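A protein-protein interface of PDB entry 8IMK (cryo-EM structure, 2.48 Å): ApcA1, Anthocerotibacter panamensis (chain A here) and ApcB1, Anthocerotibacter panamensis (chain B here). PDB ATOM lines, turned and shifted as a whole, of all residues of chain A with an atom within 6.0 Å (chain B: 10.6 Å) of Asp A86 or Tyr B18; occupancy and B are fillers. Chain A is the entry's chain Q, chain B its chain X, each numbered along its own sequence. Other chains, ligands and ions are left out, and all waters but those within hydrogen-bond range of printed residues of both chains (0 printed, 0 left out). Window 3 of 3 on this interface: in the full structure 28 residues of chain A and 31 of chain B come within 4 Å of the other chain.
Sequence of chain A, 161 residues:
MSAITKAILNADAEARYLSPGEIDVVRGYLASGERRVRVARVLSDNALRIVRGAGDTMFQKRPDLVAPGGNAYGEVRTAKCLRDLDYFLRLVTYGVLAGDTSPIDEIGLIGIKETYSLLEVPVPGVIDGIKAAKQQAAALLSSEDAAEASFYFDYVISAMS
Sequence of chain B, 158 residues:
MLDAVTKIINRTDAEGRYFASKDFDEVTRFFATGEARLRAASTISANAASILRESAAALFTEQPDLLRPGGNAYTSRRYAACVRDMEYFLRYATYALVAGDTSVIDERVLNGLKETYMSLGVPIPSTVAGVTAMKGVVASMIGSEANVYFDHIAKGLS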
ATOM      1  N   LEU A  43     -11.361 -12.016  18.051  1.00  0.00           N
ATOM      2  CA  LEU A  43      -9.981 -12.182  17.601  1.00  0.00           C
ATOM      3  C   LEU A  43      -9.873 -13.205  16.475  1.00  0.00           C
ATOM      4  O   LEU A  43      -9.061 -13.045  15.559  1.00  0.00           O
ATOM      5  CB  LEU A  43      -9.089 -12.580  18.770  1.00  0.00           C
ATOM      6  CG  LEU A  43      -8.759 -11.518  19.813  1.00  0.00           C
ATOM      7  CD1 LEU A  43      -7.747 -12.059  20.797  1.00  0.00           C
ATOM      8  CD2 LEU A  43      -8.232 -10.282  19.154  1.00  0.00           C
ATOM      9  N   SER A  44     -10.672 -14.271  16.533  1.00  0.00           N
ATOM     10  CA  SER A  44     -10.601 -15.315  15.520  1.00  0.00           C
ATOM     11  C   SER A  44     -11.201 -14.856  14.198  1.00  0.00           C
ATOM     12  O   SER A  44     -10.773 -15.298  13.128  1.00  0.00           O
ATOM     13  CB  SER A  44     -11.313 -16.570  16.021  1.00  0.00           C
ATOM     14  OG  SER A  44     -10.730 -17.043  17.216  1.00  0.00           O
ATOM     15  N   ALA A  47      -8.442 -12.653  12.242  1.00  0.00           N
ATOM     16  CA  ALA A  47      -7.066 -13.132  12.284  1.00  0.00           C
ATOM     17  C   ALA A  47      -6.260 -12.625  11.097  1.00  0.00           C
ATOM     18  O   ALA A  47      -5.114 -12.190  11.259  1.00  0.00           O
ATOM     19  CB  ALA A  47      -7.048 -14.657  12.331  1.00  0.00           C
ATOM     20  N   LEU A  48      -6.839 -12.660   9.897  1.00  0.00           N
ATOM     21  CA  LEU A  48      -6.106 -12.229   8.713  1.00  0.00           C
ATOM     22  C   LEU A  48      -5.761 -10.750   8.783  1.00  0.00           C
ATOM     23  O   LEU A  48      -4.627 -10.360   8.492  1.00  0.00           O
ATOM     24  CB  LEU A  48      -6.917 -12.528   7.456  1.00  0.00           C
ATOM     25  CG  LEU A  48      -7.453 -13.951   7.332  1.00  0.00           C
ATOM     26  CD1 LEU A  48      -8.385 -14.070   6.139  1.00  0.00           C
ATOM     27  CD2 LEU A  48      -6.311 -14.947   7.226  1.00  0.00           C
ATOM     28  N   VAL A  51      -3.020 -10.173  11.521  1.00  0.00           N
ATOM     29  CA  VAL A  51      -1.696 -10.652  11.136  1.00  0.00           C
ATOM     30  C   VAL A  51      -1.124  -9.805  10.007  1.00  0.00           C
ATOM     31  O   VAL A  51       0.074  -9.502   9.989  1.00  0.00           O
ATOM     32  CB  VAL A  51      -1.755 -12.144  10.764  1.00  0.00           C
ATOM     33  CG1 VAL A  51      -0.430 -12.608  10.214  1.00  0.00           C
ATOM     34  CG2 VAL A  51      -2.112 -12.966  11.978  1.00  0.00           C
ATOM     35  N   CYS A  81       7.523 -16.243   8.778  1.00  0.00           N
ATOM     36  CA  CYS A  81       7.382 -15.181   9.768  1.00  0.00           C
ATOM     37  C   CYS A  81       5.916 -14.805   9.989  1.00  0.00           C
ATOM     38  O   CYS A  81       5.447 -14.707  11.133  1.00  0.00           O
ATOM     39  CB  CYS A  81       8.212 -13.978   9.323  1.00  0.00           C
ATOM     40  SG  CYS A  81       7.865 -12.428  10.120  1.00  0.00           S
ATOM     41  N   LEU A  82       5.176 -14.600   8.902  1.00  0.00           N
ATOM     42  CA  LEU A  82       3.751 -14.323   9.019  1.00  0.00           C
ATOM     43  C   LEU A  82       3.013 -15.499   9.641  1.00  0.00           C
ATOM     44  O   LEU A  82       2.048 -15.320  10.391  1.00  0.00           O
ATOM     45  CB  LEU A  82       3.178 -13.994   7.645  1.00  0.00           C
ATOM     46  CG  LEU A  82       3.809 -12.768   6.996  1.00  0.00           C
ATOM     47  CD1 LEU A  82       3.077 -12.404   5.734  1.00  0.00           C
ATOM     48  CD2 LEU A  82       3.833 -11.608   7.967  1.00  0.00           C
ATOM     49  N   ARG A  83       3.461 -16.712   9.336  1.00  0.00           N
ATOM     50  CA  ARG A  83       2.873 -17.912   9.903  1.00  0.00           C
ATOM     51  C   ARG A  83       3.096 -17.975  11.407  1.00  0.00           C
ATOM     52  O   ARG A  83       2.213 -18.400  12.154  1.00  0.00           O
ATOM     53  CB  ARG A  83       3.462 -19.125   9.189  1.00  0.00           C
ATOM     54  CG  ARG A  83       2.841 -20.435   9.533  1.00  0.00           C
ATOM     55  CD  ARG A  83       3.740 -21.169  10.463  1.00  0.00           C
ATOM     56  NE  ARG A  83       4.880 -21.789   9.809  1.00  0.00           N
ATOM     57  CZ  ARG A  83       6.073 -21.927  10.373  1.00  0.00           C
ATOM     58  NH1 ARG A  83       6.302 -21.442  11.577  1.00  0.00           N
ATOM     59  NH2 ARG A  83       7.047 -22.523   9.716  1.00  0.00           N
ATOM     60  N   ASP A  84       4.269 -17.551  11.869  1.00  0.00           N
ATOM     61  CA  ASP A  84       4.536 -17.493  13.302  1.00  0.00           C
ATOM     62  C   ASP A  84       3.662 -16.458  13.990  1.00  0.00           C
ATOM     63  O   ASP A  84       3.192 -16.676  15.111  1.00  0.00           O
ATOM     64  CB  ASP A  84       6.005 -17.177  13.544  1.00  0.00           C
ATOM     65  CG  ASP A  84       6.869 -18.388  13.464  1.00  0.00           C
ATOM     66  OD1 ASP A  84       6.422 -19.400  12.892  1.00  0.00           O
ATOM     67  OD2 ASP A  84       8.001 -18.329  13.968  1.00  0.00           O
ATOM     68  N   LEU A  85       3.460 -15.308  13.346  1.00  0.00           N
ATOM     69  CA  LEU A  85       2.560 -14.309  13.913  1.00  0.00           C
ATOM     70  C   LEU A  85       1.139 -14.849  14.019  1.00  0.00           C
ATOM     71  O   LEU A  85       0.456 -14.648  15.034  1.00  0.00           O
ATOM     72  CB  LEU A  85       2.595 -13.038  13.071  1.00  0.00           C
ATOM     73  CG  LEU A  85       3.881 -12.227  13.215  1.00  0.00           C
ATOM     74  CD1 LEU A  85       3.926 -11.129  12.179  1.00  0.00           C
ATOM     75  CD2 LEU A  85       4.001 -11.657  14.610  1.00  0.00           C
ATOM     76  N   ASP A  86       0.685 -15.552  12.984  1.00  0.00           N
ATOM     77  CA  ASP A  86      -0.628 -16.180  13.026  1.00  0.00           C
ATOM     78  C   ASP A  86      -0.696 -17.219  14.143  1.00  0.00           C
ATOM     79  O   ASP A  86      -1.710 -17.328  14.844  1.00  0.00           O
ATOM     80  CB  ASP A  86      -0.921 -16.803  11.664  1.00  0.00           C
ATOM     81  CG  ASP A  86      -2.340 -17.295  11.532  1.00  0.00           C
ATOM     82  OD1 ASP A  86      -3.108 -17.185  12.502  1.00  0.00           O
ATOM     83  OD2 ASP A  86      -2.693 -17.806  10.451  1.00  0.00           O
ATOM     84  N   TYR A  87       0.381 -17.983  14.324  1.00  0.00           N
ATOM     85  CA  TYR A  87       0.449 -18.964  15.401  1.00  0.00           C
ATOM     86  C   TYR A  87       0.281 -18.305  16.758  1.00  0.00           C
ATOM     87  O   TYR A  87      -0.471 -18.795  17.608  1.00  0.00           O
ATOM     88  CB  TYR A  87       1.787 -19.694  15.362  1.00  0.00           C
ATOM     89  CG  TYR A  87       1.870 -20.855  14.412  1.00  0.00           C
ATOM     90  CD1 TYR A  87       0.765 -21.283  13.706  1.00  0.00           C
ATOM     91  CD2 TYR A  87       3.065 -21.525  14.227  1.00  0.00           C
ATOM     92  CE1 TYR A  87       0.844 -22.343  12.847  1.00  0.00           C
ATOM     93  CE2 TYR A  87       3.151 -22.593  13.383  1.00  0.00           C
ATOM     94  CZ  TYR A  87       2.041 -22.996  12.683  1.00  0.00           C
ATOM     95  OH  TYR A  87       2.129 -24.061  11.822  1.00  0.00           O
ATOM     96  N   PHE A  88       0.988 -17.202  16.986  1.00  0.00           N
ATOM     97  CA  PHE A  88       0.931 -16.558  18.290  1.00  0.00           C
ATOM     98  C   PHE A  88      -0.428 -15.920  18.536  1.00  0.00           C
ATOM     99  O   PHE A  88      -0.926 -15.929  19.667  1.00  0.00           O
ATOM    100  CB  PHE A  88       2.059 -15.538  18.417  1.00  0.00           C
ATOM    101  CG  PHE A  88       3.404 -16.164  18.606  1.00  0.00           C
ATOM    102  CD1 PHE A  88       3.613 -17.091  19.604  1.00  0.00           C
ATOM    103  CD2 PHE A  88       4.455 -15.843  17.769  1.00  0.00           C
ATOM    104  CE1 PHE A  88       4.844 -17.672  19.773  1.00  0.00           C
ATOM    105  CE2 PHE A  88       5.687 -16.425  17.934  1.00  0.00           C
ATOM    106  CZ  PHE A  88       5.882 -17.341  18.936  1.00  0.00           C
ATOM    107  N   LEU A  89      -1.058 -15.377  17.492  1.00  0.00           N
ATOM    108  CA  LEU A  89      -2.420 -14.875  17.650  1.00  0.00           C
ATOM    109  C   LEU A  89      -3.391 -15.998  18.014  1.00  0.00           C
ATOM    110  O   LEU A  89      -4.242 -15.838  18.901  1.00  0.00           O
ATOM    111  CB  LEU A  89      -2.869 -14.167  16.375  1.00  0.00           C
ATOM    112  CG  LEU A  89      -4.280 -13.589  16.430  1.00  0.00           C
ATOM    113  CD1 LEU A  89      -4.342 -12.415  17.377  1.00  0.00           C
ATOM    114  CD2 LEU A  89      -4.750 -13.193  15.061  1.00  0.00           C
ATOM    115  N   ARG A  90      -3.274 -17.144  17.345  1.00  0.00           N
ATOM    116  CA  ARG A  90      -4.123 -18.283  17.682  1.00  0.00           C
ATOM    117  C   ARG A  90      -3.896 -18.736  19.117  1.00  0.00           C
ATOM    118  O   ARG A  90      -4.843 -19.096  19.826  1.00  0.00           O
ATOM    119  CB  ARG A  90      -3.853 -19.426  16.711  1.00  0.00           C
ATOM    120  CG  ARG A  90      -4.768 -20.591  16.886  1.00  0.00           C
ATOM    121  CD  ARG A  90      -4.952 -21.332  15.596  1.00  0.00           C
ATOM    122  NE  ARG A  90      -3.686 -21.783  15.034  1.00  0.00           N
ATOM    123  CZ  ARG A  90      -3.044 -22.882  15.412  1.00  0.00           C
ATOM    124  NH1 ARG A  90      -3.539 -23.653  16.366  1.00  0.00           N
ATOM    125  NH2 ARG A  90      -1.900 -23.203  14.841  1.00  0.00           N
ATOM    126  N   LEU A  91      -2.642 -18.731  19.561  1.00  0.00           N
ATOM    127  CA  LEU A  91      -2.341 -19.137  20.926  1.00  0.00           C
ATOM    128  C   LEU A  91      -2.898 -18.143  21.931  1.00  0.00           C
ATOM    129  O   LEU A  91      -3.293 -18.523  23.034  1.00  0.00           O
ATOM    130  CB  LEU A  91      -0.837 -19.295  21.100  1.00  0.00           C
ATOM    131  CG  LEU A  91      -0.221 -20.468  20.351  1.00  0.00           C
ATOM    132  CD1 LEU A  91       1.110 -20.790  20.952  1.00  0.00           C
ATOM    133  CD2 LEU A  91      -1.132 -21.668  20.402  1.00  0.00           C
ATOM    134  N   THR A  93      -5.678 -16.447  21.483  1.00  0.00           N
ATOM    135  CA  THR A  93      -7.092 -16.815  21.581  1.00  0.00           C
ATOM    136  C   THR A  93      -7.285 -18.036  22.476  1.00  0.00           C
ATOM    137  O   THR A  93      -8.241 -18.101  23.261  1.00  0.00           O
ATOM    138  CB  THR A  93      -7.681 -17.077  20.198  1.00  0.00           C
ATOM    139  OG1 THR A  93      -6.882 -18.045  19.516  1.00  0.00           O
ATOM    140  CG2 THR A  93      -7.713 -15.811  19.391  1.00  0.00           C
ATOM    141  N   TYR A  94      -6.386 -19.015  22.368  1.00  0.00           N
ATOM    142  CA  TYR A  94      -6.457 -20.183  23.243  1.00  0.00           C
ATOM    143  C   TYR A  94      -6.310 -19.794  24.706  1.00  0.00           C
ATOM    144  O   TYR A  94      -7.039 -20.296  25.563  1.00  0.00           O
ATOM    145  CB  TYR A  94      -5.379 -21.196  22.873  1.00  0.00           C
ATOM    146  CG  TYR A  94      -5.583 -21.864  21.551  1.00  0.00           C
ATOM    147  CD1 TYR A  94      -6.774 -21.732  20.863  1.00  0.00           C
ATOM    148  CD2 TYR A  94      -4.586 -22.638  20.991  1.00  0.00           C
ATOM    149  CE1 TYR A  94      -6.956 -22.344  19.656  1.00  0.00           C
ATOM    150  CE2 TYR A  94      -4.766 -23.259  19.788  1.00  0.00           C
ATOM    151  CZ  TYR A  94      -5.948 -23.108  19.123  1.00  0.00           C
ATOM    152  OH  TYR A  94      -6.122 -23.725  17.914  1.00  0.00           O
ATOM    153  N   ILE B   8     -11.184 -29.151  23.469  1.00  0.00           N
ATOM    154  CA  ILE B   8     -11.544 -28.426  22.254  1.00  0.00           C
ATOM    155  C   ILE B   8     -10.340 -27.674  21.695  1.00  0.00           C
ATOM    156  O   ILE B   8     -10.111 -27.648  20.477  1.00  0.00           O
ATOM    157  CB  ILE B   8     -12.724 -27.481  22.533  1.00  0.00           C
ATOM    158  CG1 ILE B   8     -13.858 -28.238  23.213  1.00  0.00           C
ATOM    159  CG2 ILE B   8     -13.218 -26.840  21.254  1.00  0.00           C
ATOM    160  CD1 ILE B   8     -14.906 -27.342  23.792  1.00  0.00           C
ATOM    161  N   ILE B   9      -9.568 -27.035  22.575  1.00  0.00           N
ATOM    162  CA  ILE B   9      -8.375 -26.314  22.149  1.00  0.00           C
ATOM    163  C   ILE B   9      -7.384 -27.261  21.493  1.00  0.00           C
ATOM    164  O   ILE B   9      -6.801 -26.945  20.450  1.00  0.00           O
ATOM    165  CB  ILE B   9      -7.734 -25.581  23.340  1.00  0.00           C
ATOM    166  CG1 ILE B   9      -8.580 -24.394  23.766  1.00  0.00           C
ATOM    167  CG2 ILE B   9      -6.345 -25.104  22.986  1.00  0.00           C
ATOM    168  CD1 ILE B   9      -8.090 -23.752  25.023  1.00  0.00           C
ATOM    169  N   ASN B  10      -7.171 -28.430  22.093  1.00  0.00           N
ATOM    170  CA  ASN B  10      -6.241 -29.398  21.530  1.00  0.00           C
ATOM    171  C   ASN B  10      -6.707 -29.871  20.166  1.00  0.00           C
ATOM    172  O   ASN B  10      -5.900 -30.009  19.242  1.00  0.00           O
ATOM    173  CB  ASN B  10      -6.083 -30.582  22.480  1.00  0.00           C
ATOM    174  CG  ASN B  10      -5.139 -30.288  23.620  1.00  0.00           C
ATOM    175  OD1 ASN B  10      -4.720 -29.153  23.815  1.00  0.00           O
ATOM    176  ND2 ASN B  10      -4.810 -31.308  24.389  1.00  0.00           N
ATOM    177  N   ARG B  11      -8.008 -30.116  20.018  1.00  0.00           N
ATOM    178  CA  ARG B  11      -8.537 -30.534  18.726  1.00  0.00           C
ATOM    179  C   ARG B  11      -8.270 -29.481  17.659  1.00  0.00           C
ATOM    180  O   ARG B  11      -7.709 -29.779  16.596  1.00  0.00           O
ATOM    181  CB  ARG B  11     -10.032 -30.807  18.846  1.00  0.00           C
ATOM    182  CG  ARG B  11     -10.627 -31.483  17.640  1.00  0.00           C
ATOM    183  CD  ARG B  11     -11.968 -32.107  17.952  1.00  0.00           C
ATOM    184  NE  ARG B  11     -12.960 -31.149  18.420  1.00  0.00           N
ATOM    185  CZ  ARG B  11     -13.538 -31.204  19.614  1.00  0.00           C
ATOM    186  NH1 ARG B  11     -13.213 -32.168  20.461  1.00  0.00           N
ATOM    187  NH2 ARG B  11     -14.435 -30.295  19.959  1.00  0.00           N
ATOM    188  N   THR B  12      -8.652 -28.233  17.934  1.00  0.00           N
ATOM    189  CA  THR B  12      -8.467 -27.183  16.939  1.00  0.00           C
ATOM    190  C   THR B  12      -6.993 -26.963  16.632  1.00  0.00           C
ATOM    191  O   THR B  12      -6.623 -26.728  15.478  1.00  0.00           O
ATOM    192  CB  THR B  12      -9.117 -25.882  17.401  1.00  0.00           C
ATOM    193  OG1 THR B  12      -8.654 -25.549  18.712  1.00  0.00           O
ATOM    194  CG2 THR B  12     -10.612 -26.030  17.429  1.00  0.00           C
ATOM    195  N   ASP B  13      -6.138 -27.030  17.651  1.00  0.00           N
ATOM    196  CA  ASP B  13      -4.711 -26.833  17.440  1.00  0.00           C
ATOM    197  C   ASP B  13      -4.115 -27.943  16.587  1.00  0.00           C
ATOM    198  O   ASP B  13      -3.262 -27.684  15.731  1.00  0.00           O
ATOM    199  CB  ASP B  13      -4.005 -26.734  18.787  1.00  0.00           C
ATOM    200  CG  ASP B  13      -2.511 -26.730  18.656  1.00  0.00           C
ATOM    201  OD1 ASP B  13      -1.935 -25.632  18.534  1.00  0.00           O
ATOM    202  OD2 ASP B  13      -1.907 -27.819  18.689  1.00  0.00           O
ATOM    203  N   ALA B  14      -4.544 -29.188  16.805  1.00  0.00           N
ATOM    204  CA  ALA B  14      -4.074 -30.281  15.963  1.00  0.00           C
ATOM    205  C   ALA B  14      -4.561 -30.119  14.531  1.00  0.00           C
ATOM    206  O   ALA B  14      -3.890 -30.550  13.589  1.00  0.00           O
ATOM    207  CB  ALA B  14      -4.526 -31.622  16.538  1.00  0.00           C
ATOM    208  N   GLU B  15      -5.731 -29.515  14.343  1.00  0.00           N
ATOM    209  CA  GLU B  15      -6.117 -29.146  12.987  1.00  0.00           C
ATOM    210  C   GLU B  15      -5.468 -27.854  12.520  1.00  0.00           C
ATOM    211  O   GLU B  15      -5.563 -27.527  11.335  1.00  0.00           O
ATOM    212  CB  GLU B  15      -7.635 -29.037  12.870  1.00  0.00           C
ATOM    213  CG  GLU B  15      -8.377 -30.128  13.605  1.00  0.00           C
ATOM    214  CD  GLU B  15      -9.862 -29.869  13.694  1.00  0.00           C
ATOM    215  OE1 GLU B  15     -10.641 -30.653  13.115  1.00  0.00           O
ATOM    216  OE2 GLU B  15     -10.251 -28.888  14.358  1.00  0.00           O
ATOM    217  N   GLY B  16      -4.803 -27.127  13.410  1.00  0.00           N
ATOM    218  CA  GLY B  16      -4.130 -25.901  13.031  1.00  0.00           C
ATOM    219  C   GLY B  16      -5.070 -24.801  12.605  1.00  0.00           C
ATOM    220  O   GLY B  16      -4.756 -24.040  11.685  1.00  0.00           O
ATOM    221  N   ARG B  17      -6.217 -24.687  13.261  1.00  0.00           N
ATOM    222  CA  ARG B  17      -7.215 -23.702  12.888  1.00  0.00           C
ATOM    223  C   ARG B  17      -7.681 -22.939  14.116  1.00  0.00           C
ATOM    224  O   ARG B  17      -7.534 -23.393  15.252  1.00  0.00           O
ATOM    225  CB  ARG B  17      -8.416 -24.350  12.190  1.00  0.00           C
ATOM    226  CG  ARG B  17      -9.092 -25.427  12.997  1.00  0.00           C
ATOM    227  CD  ARG B  17     -10.391 -25.834  12.355  1.00  0.00           C
ATOM    228  NE  ARG B  17     -11.093 -26.834  13.149  1.00  0.00           N
ATOM    229  CZ  ARG B  17     -11.993 -26.547  14.081  1.00  0.00           C
ATOM    230  NH1 ARG B  17     -12.300 -25.287  14.344  1.00  0.00           N
ATOM    231  NH2 ARG B  17     -12.576 -27.523  14.758  1.00  0.00           N
ATOM    232  N   TYR B  18      -8.214 -21.751  13.867  1.00  0.00           N
ATOM    233  CA  TYR B  18      -8.844 -20.974  14.916  1.00  0.00           C
ATOM    234  C   TYR B  18     -10.171 -21.609  15.312  1.00  0.00           C
ATOM    235  O   TYR B  18     -10.723 -22.456  14.607  1.00  0.00           O
ATOM    236  CB  TYR B  18      -9.074 -19.536  14.454  1.00  0.00           C
ATOM    237  CG  TYR B  18      -7.829 -18.692  14.413  1.00  0.00           C
ATOM    238  CD1 TYR B  18      -6.910 -18.843  13.394  1.00  0.00           C
ATOM    239  CD2 TYR B  18      -7.573 -17.747  15.389  1.00  0.00           C
ATOM    240  CE1 TYR B  18      -5.776 -18.084  13.347  1.00  0.00           C
ATOM    241  CE2 TYR B  18      -6.443 -16.976  15.349  1.00  0.00           C
ATOM    242  CZ  TYR B  18      -5.543 -17.150  14.326  1.00  0.00           C
ATOM    243  OH  TYR B  18      -4.403 -16.387  14.277  1.00  0.00           O
ATOM    244  N   PHE B  19     -10.678 -21.196  16.465  1.00  0.00           N
ATOM    245  CA  PHE B  19     -12.017 -21.595  16.864  1.00  0.00           C
ATOM    246  C   PHE B  19     -13.036 -21.087  15.853  1.00  0.00           C
ATOM    247  O   PHE B  19     -12.941 -19.961  15.362  1.00  0.00           O
ATOM    248  CB  PHE B  19     -12.334 -21.038  18.246  1.00  0.00           C
ATOM    249  CG  PHE B  19     -12.029 -21.975  19.368  1.00  0.00           C
ATOM    250  CD1 PHE B  19     -10.744 -22.433  19.575  1.00  0.00           C
ATOM    251  CD2 PHE B  19     -13.023 -22.373  20.236  1.00  0.00           C
ATOM    252  CE1 PHE B  19     -10.459 -23.283  20.611  1.00  0.00           C
ATOM    253  CE2 PHE B  19     -12.744 -23.227  21.278  1.00  0.00           C
ATOM    254  CZ  PHE B  19     -11.458 -23.679  21.465  1.00  0.00           C
ATOM    255  N   ALA B  20     -14.008 -21.925  15.537  1.00  0.00           N
ATOM    256  CA  ALA B  20     -15.126 -21.565  14.683  1.00  0.00           C
ATOM    257  C   ALA B  20     -16.403 -21.535  15.515  1.00  0.00           C
ATOM    258  O   ALA B  20     -16.381 -21.693  16.736  1.00  0.00           O
ATOM    259  CB  ALA B  20     -15.245 -22.537  13.509  1.00  0.00           C
ATOM    260  N   SER B  21     -17.533 -21.337  14.836  1.00  0.00           N
ATOM    261  CA  SER B  21     -18.802 -21.192  15.542  1.00  0.00           C
ATOM    262  C   SER B  21     -19.156 -22.446  16.333  1.00  0.00           C
ATOM    263  O   SER B  21     -19.615 -22.351  17.473  1.00  0.00           O
ATOM    264  CB  SER B  21     -19.913 -20.853  14.551  1.00  0.00           C
ATOM    265  OG  SER B  21     -19.670 -19.606  13.928  1.00  0.00           O
ATOM    266  N   LYS B  22     -18.937 -23.626  15.752  1.00  0.00           N
ATOM    267  CA  LYS B  22     -19.301 -24.868  16.428  1.00  0.00           C
ATOM    268  C   LYS B  22     -18.505 -25.060  17.715  1.00  0.00           C
ATOM    269  O   LYS B  22     -19.057 -25.472  18.746  1.00  0.00           O
ATOM    270  CB  LYS B  22     -19.089 -26.045  15.478  1.00  0.00           C
ATOM    271  CG  LYS B  22     -19.677 -27.355  15.951  1.00  0.00           C
ATOM    272  CD  LYS B  22     -21.159 -27.227  16.255  1.00  0.00           C
ATOM    273  CE  LYS B  22     -21.725 -28.548  16.748  1.00  0.00           C
ATOM    274  NZ  LYS B  22     -21.918 -29.519  15.634  1.00  0.00           N
ATOM    275  N   ASP B  23     -17.206 -24.758  17.679  1.00  0.00           N
ATOM    276  CA  ASP B  23     -16.382 -24.872  18.876  1.00  0.00           C
ATOM    277  C   ASP B  23     -16.813 -23.873  19.939  1.00  0.00           C
ATOM    278  O   ASP B  23     -16.792 -24.180  21.136  1.00  0.00           O
ATOM    279  CB  ASP B  23     -14.912 -24.677  18.517  1.00  0.00           C
ATOM    280  CG  ASP B  23     -14.528 -25.380  17.237  1.00  0.00           C
ATOM    281  OD1 ASP B  23     -13.986 -24.715  16.333  1.00  0.00           O
ATOM    282  OD2 ASP B  23     -14.755 -26.602  17.137  1.00  0.00           O
ATOM    283  N   PHE B  24     -17.197 -22.668  19.524  1.00  0.00           N
ATOM    284  CA  PHE B  24     -17.677 -21.683  20.483  1.00  0.00           C
ATOM    285  C   PHE B  24     -18.990 -22.122  21.112  1.00  0.00           C
ATOM    286  O   PHE B  24     -19.205 -21.921  22.310  1.00  0.00           O
ATOM    287  CB  PHE B  24     -17.820 -20.319  19.813  1.00  0.00           C
ATOM    288  CG  PHE B  24     -16.516 -19.616  19.602  1.00  0.00           C
ATOM    289  CD1 PHE B  24     -15.639 -19.434  20.653  1.00  0.00           C
ATOM    290  CD2 PHE B  24     -16.160 -19.145  18.356  1.00  0.00           C
ATOM    291  CE1 PHE B  24     -14.437 -18.787  20.461  1.00  0.00           C
ATOM    292  CE2 PHE B  24     -14.960 -18.497  18.163  1.00  0.00           C
ATOM    293  CZ  PHE B  24     -14.097 -18.325  19.213  1.00  0.00           C
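Among the printed residues, merely in contact across the chains: Ser A44 with Tyr B18, Ser A44 with Phe B19, Ala A47 with Tyr B18, Leu A89 with Tyr B18, Arg A90 with Gly B16, Arg A90 with Arg B17, Tyr A94 with Ile B9 and Tyr A94 with Phe B19.
Of chain B, only Tyr B18 and Phe B19 come within 4 Å of Ser A44. Ala A47 touches just one residue of chain B: Tyr B18 (3.5 Å). Leu A85 touches none of the printed residues of chain B. Of chain B, only Tyr B18 (2.3 Å) comes within 4 Å of Asp A86. Leu A89 touches just one residue of chain B: Tyr B18 (3.3 Å). Arg A90 touches just these residues of chain B: Asp B13 (3.3 Å), Gly B16 (3.9 Å), Arg B17 (3.3 Å) and Tyr B18 (3.4 Å). Arg B11 touches none of the printed residues of chain A. Of the printed residues of chain A, Thr B12 touches Tyr A94 (3.2 Å). Printed residues of chain A within 4 Å of Gly B16: Arg A90 (3.9 Å). Of chain A, only Ser A44, Ala A47, Asp A86, Leu A89 and Arg A90 come within 4 Å of Tyr B18. The nearest printed residue of chain A that does not touch Gly B16 is Tyr A94 (5.5 Å).
The backbone carbonyl oxygen (O) of Asp A86 lies within hydrogen-bond range of the side-chain hydroxyl (OH) of Tyr B18. The side-chain carboxylate (OD1) of Asp B13 lies within salt-bridge range of the guanidinium group (NH1) of Arg A90 (3.3 Å). The backbone NH of Arg A90 lies within hydrogen-bond range of the side-chain hydroxyl of Tyr B18, at 3.4 Å. The side-chain hydroxyl (OH) of Tyr A94 is in hydrogen-bond range of the side-chain hydroxyl (OG1) of Thr B12, at 3.2 Å. The side-chain hydroxyl (OH) of Tyr A94 lies within hydrogen-bond range of the backbone NH (N) of Asp B13, 3.3 Å away. The backbone carbonyl oxygen of Arg B17 lies within hydrogen-bond range of the side-chain hydroxyl of Tyr A94 (3.0 Å).
Of the 17 printed residues of chain B, 7 touch a printed residue of chain A. Hydrophobic or aromatic side chains of chain B within 4 Å of the printed part of chain A: Ile B9, Tyr B18 and Phe B19. Among the printed residues, 14 pairs touch across the chains.
The backbone carbonyl oxygen (O) of Leu A89 is in hydrogen-bond range of the side-chain hydroxyl (OG1) of Thr A93 (3.5 Å). The guanidinium group (NH1) of Arg A90 lies within hydrogen-bond range of the side-chain hydroxyl (OH) of Tyr A94 (3.0 Å). The backbone carbonyl oxygen (O) of Ile B8 is in hydrogen-bond range of the side-chain hydroxyl (OG1) of Thr B12, at 3.1 Å. The backbone carbonyl oxygen (O) of Ile B9 sits at hydrogen-bond distance from the side-chain hydroxyl (OG1) of Thr B12 (2.9 Å). The backbone NH of Arg B17 sits at hydrogen-bond distance from the backbone carbonyl oxygen of Thr B12. The guanidinium group (NE) of Arg B17 lies within salt-bridge range of the side-chain carboxylate (OE2) of Glu B15, 2.5 Å away.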
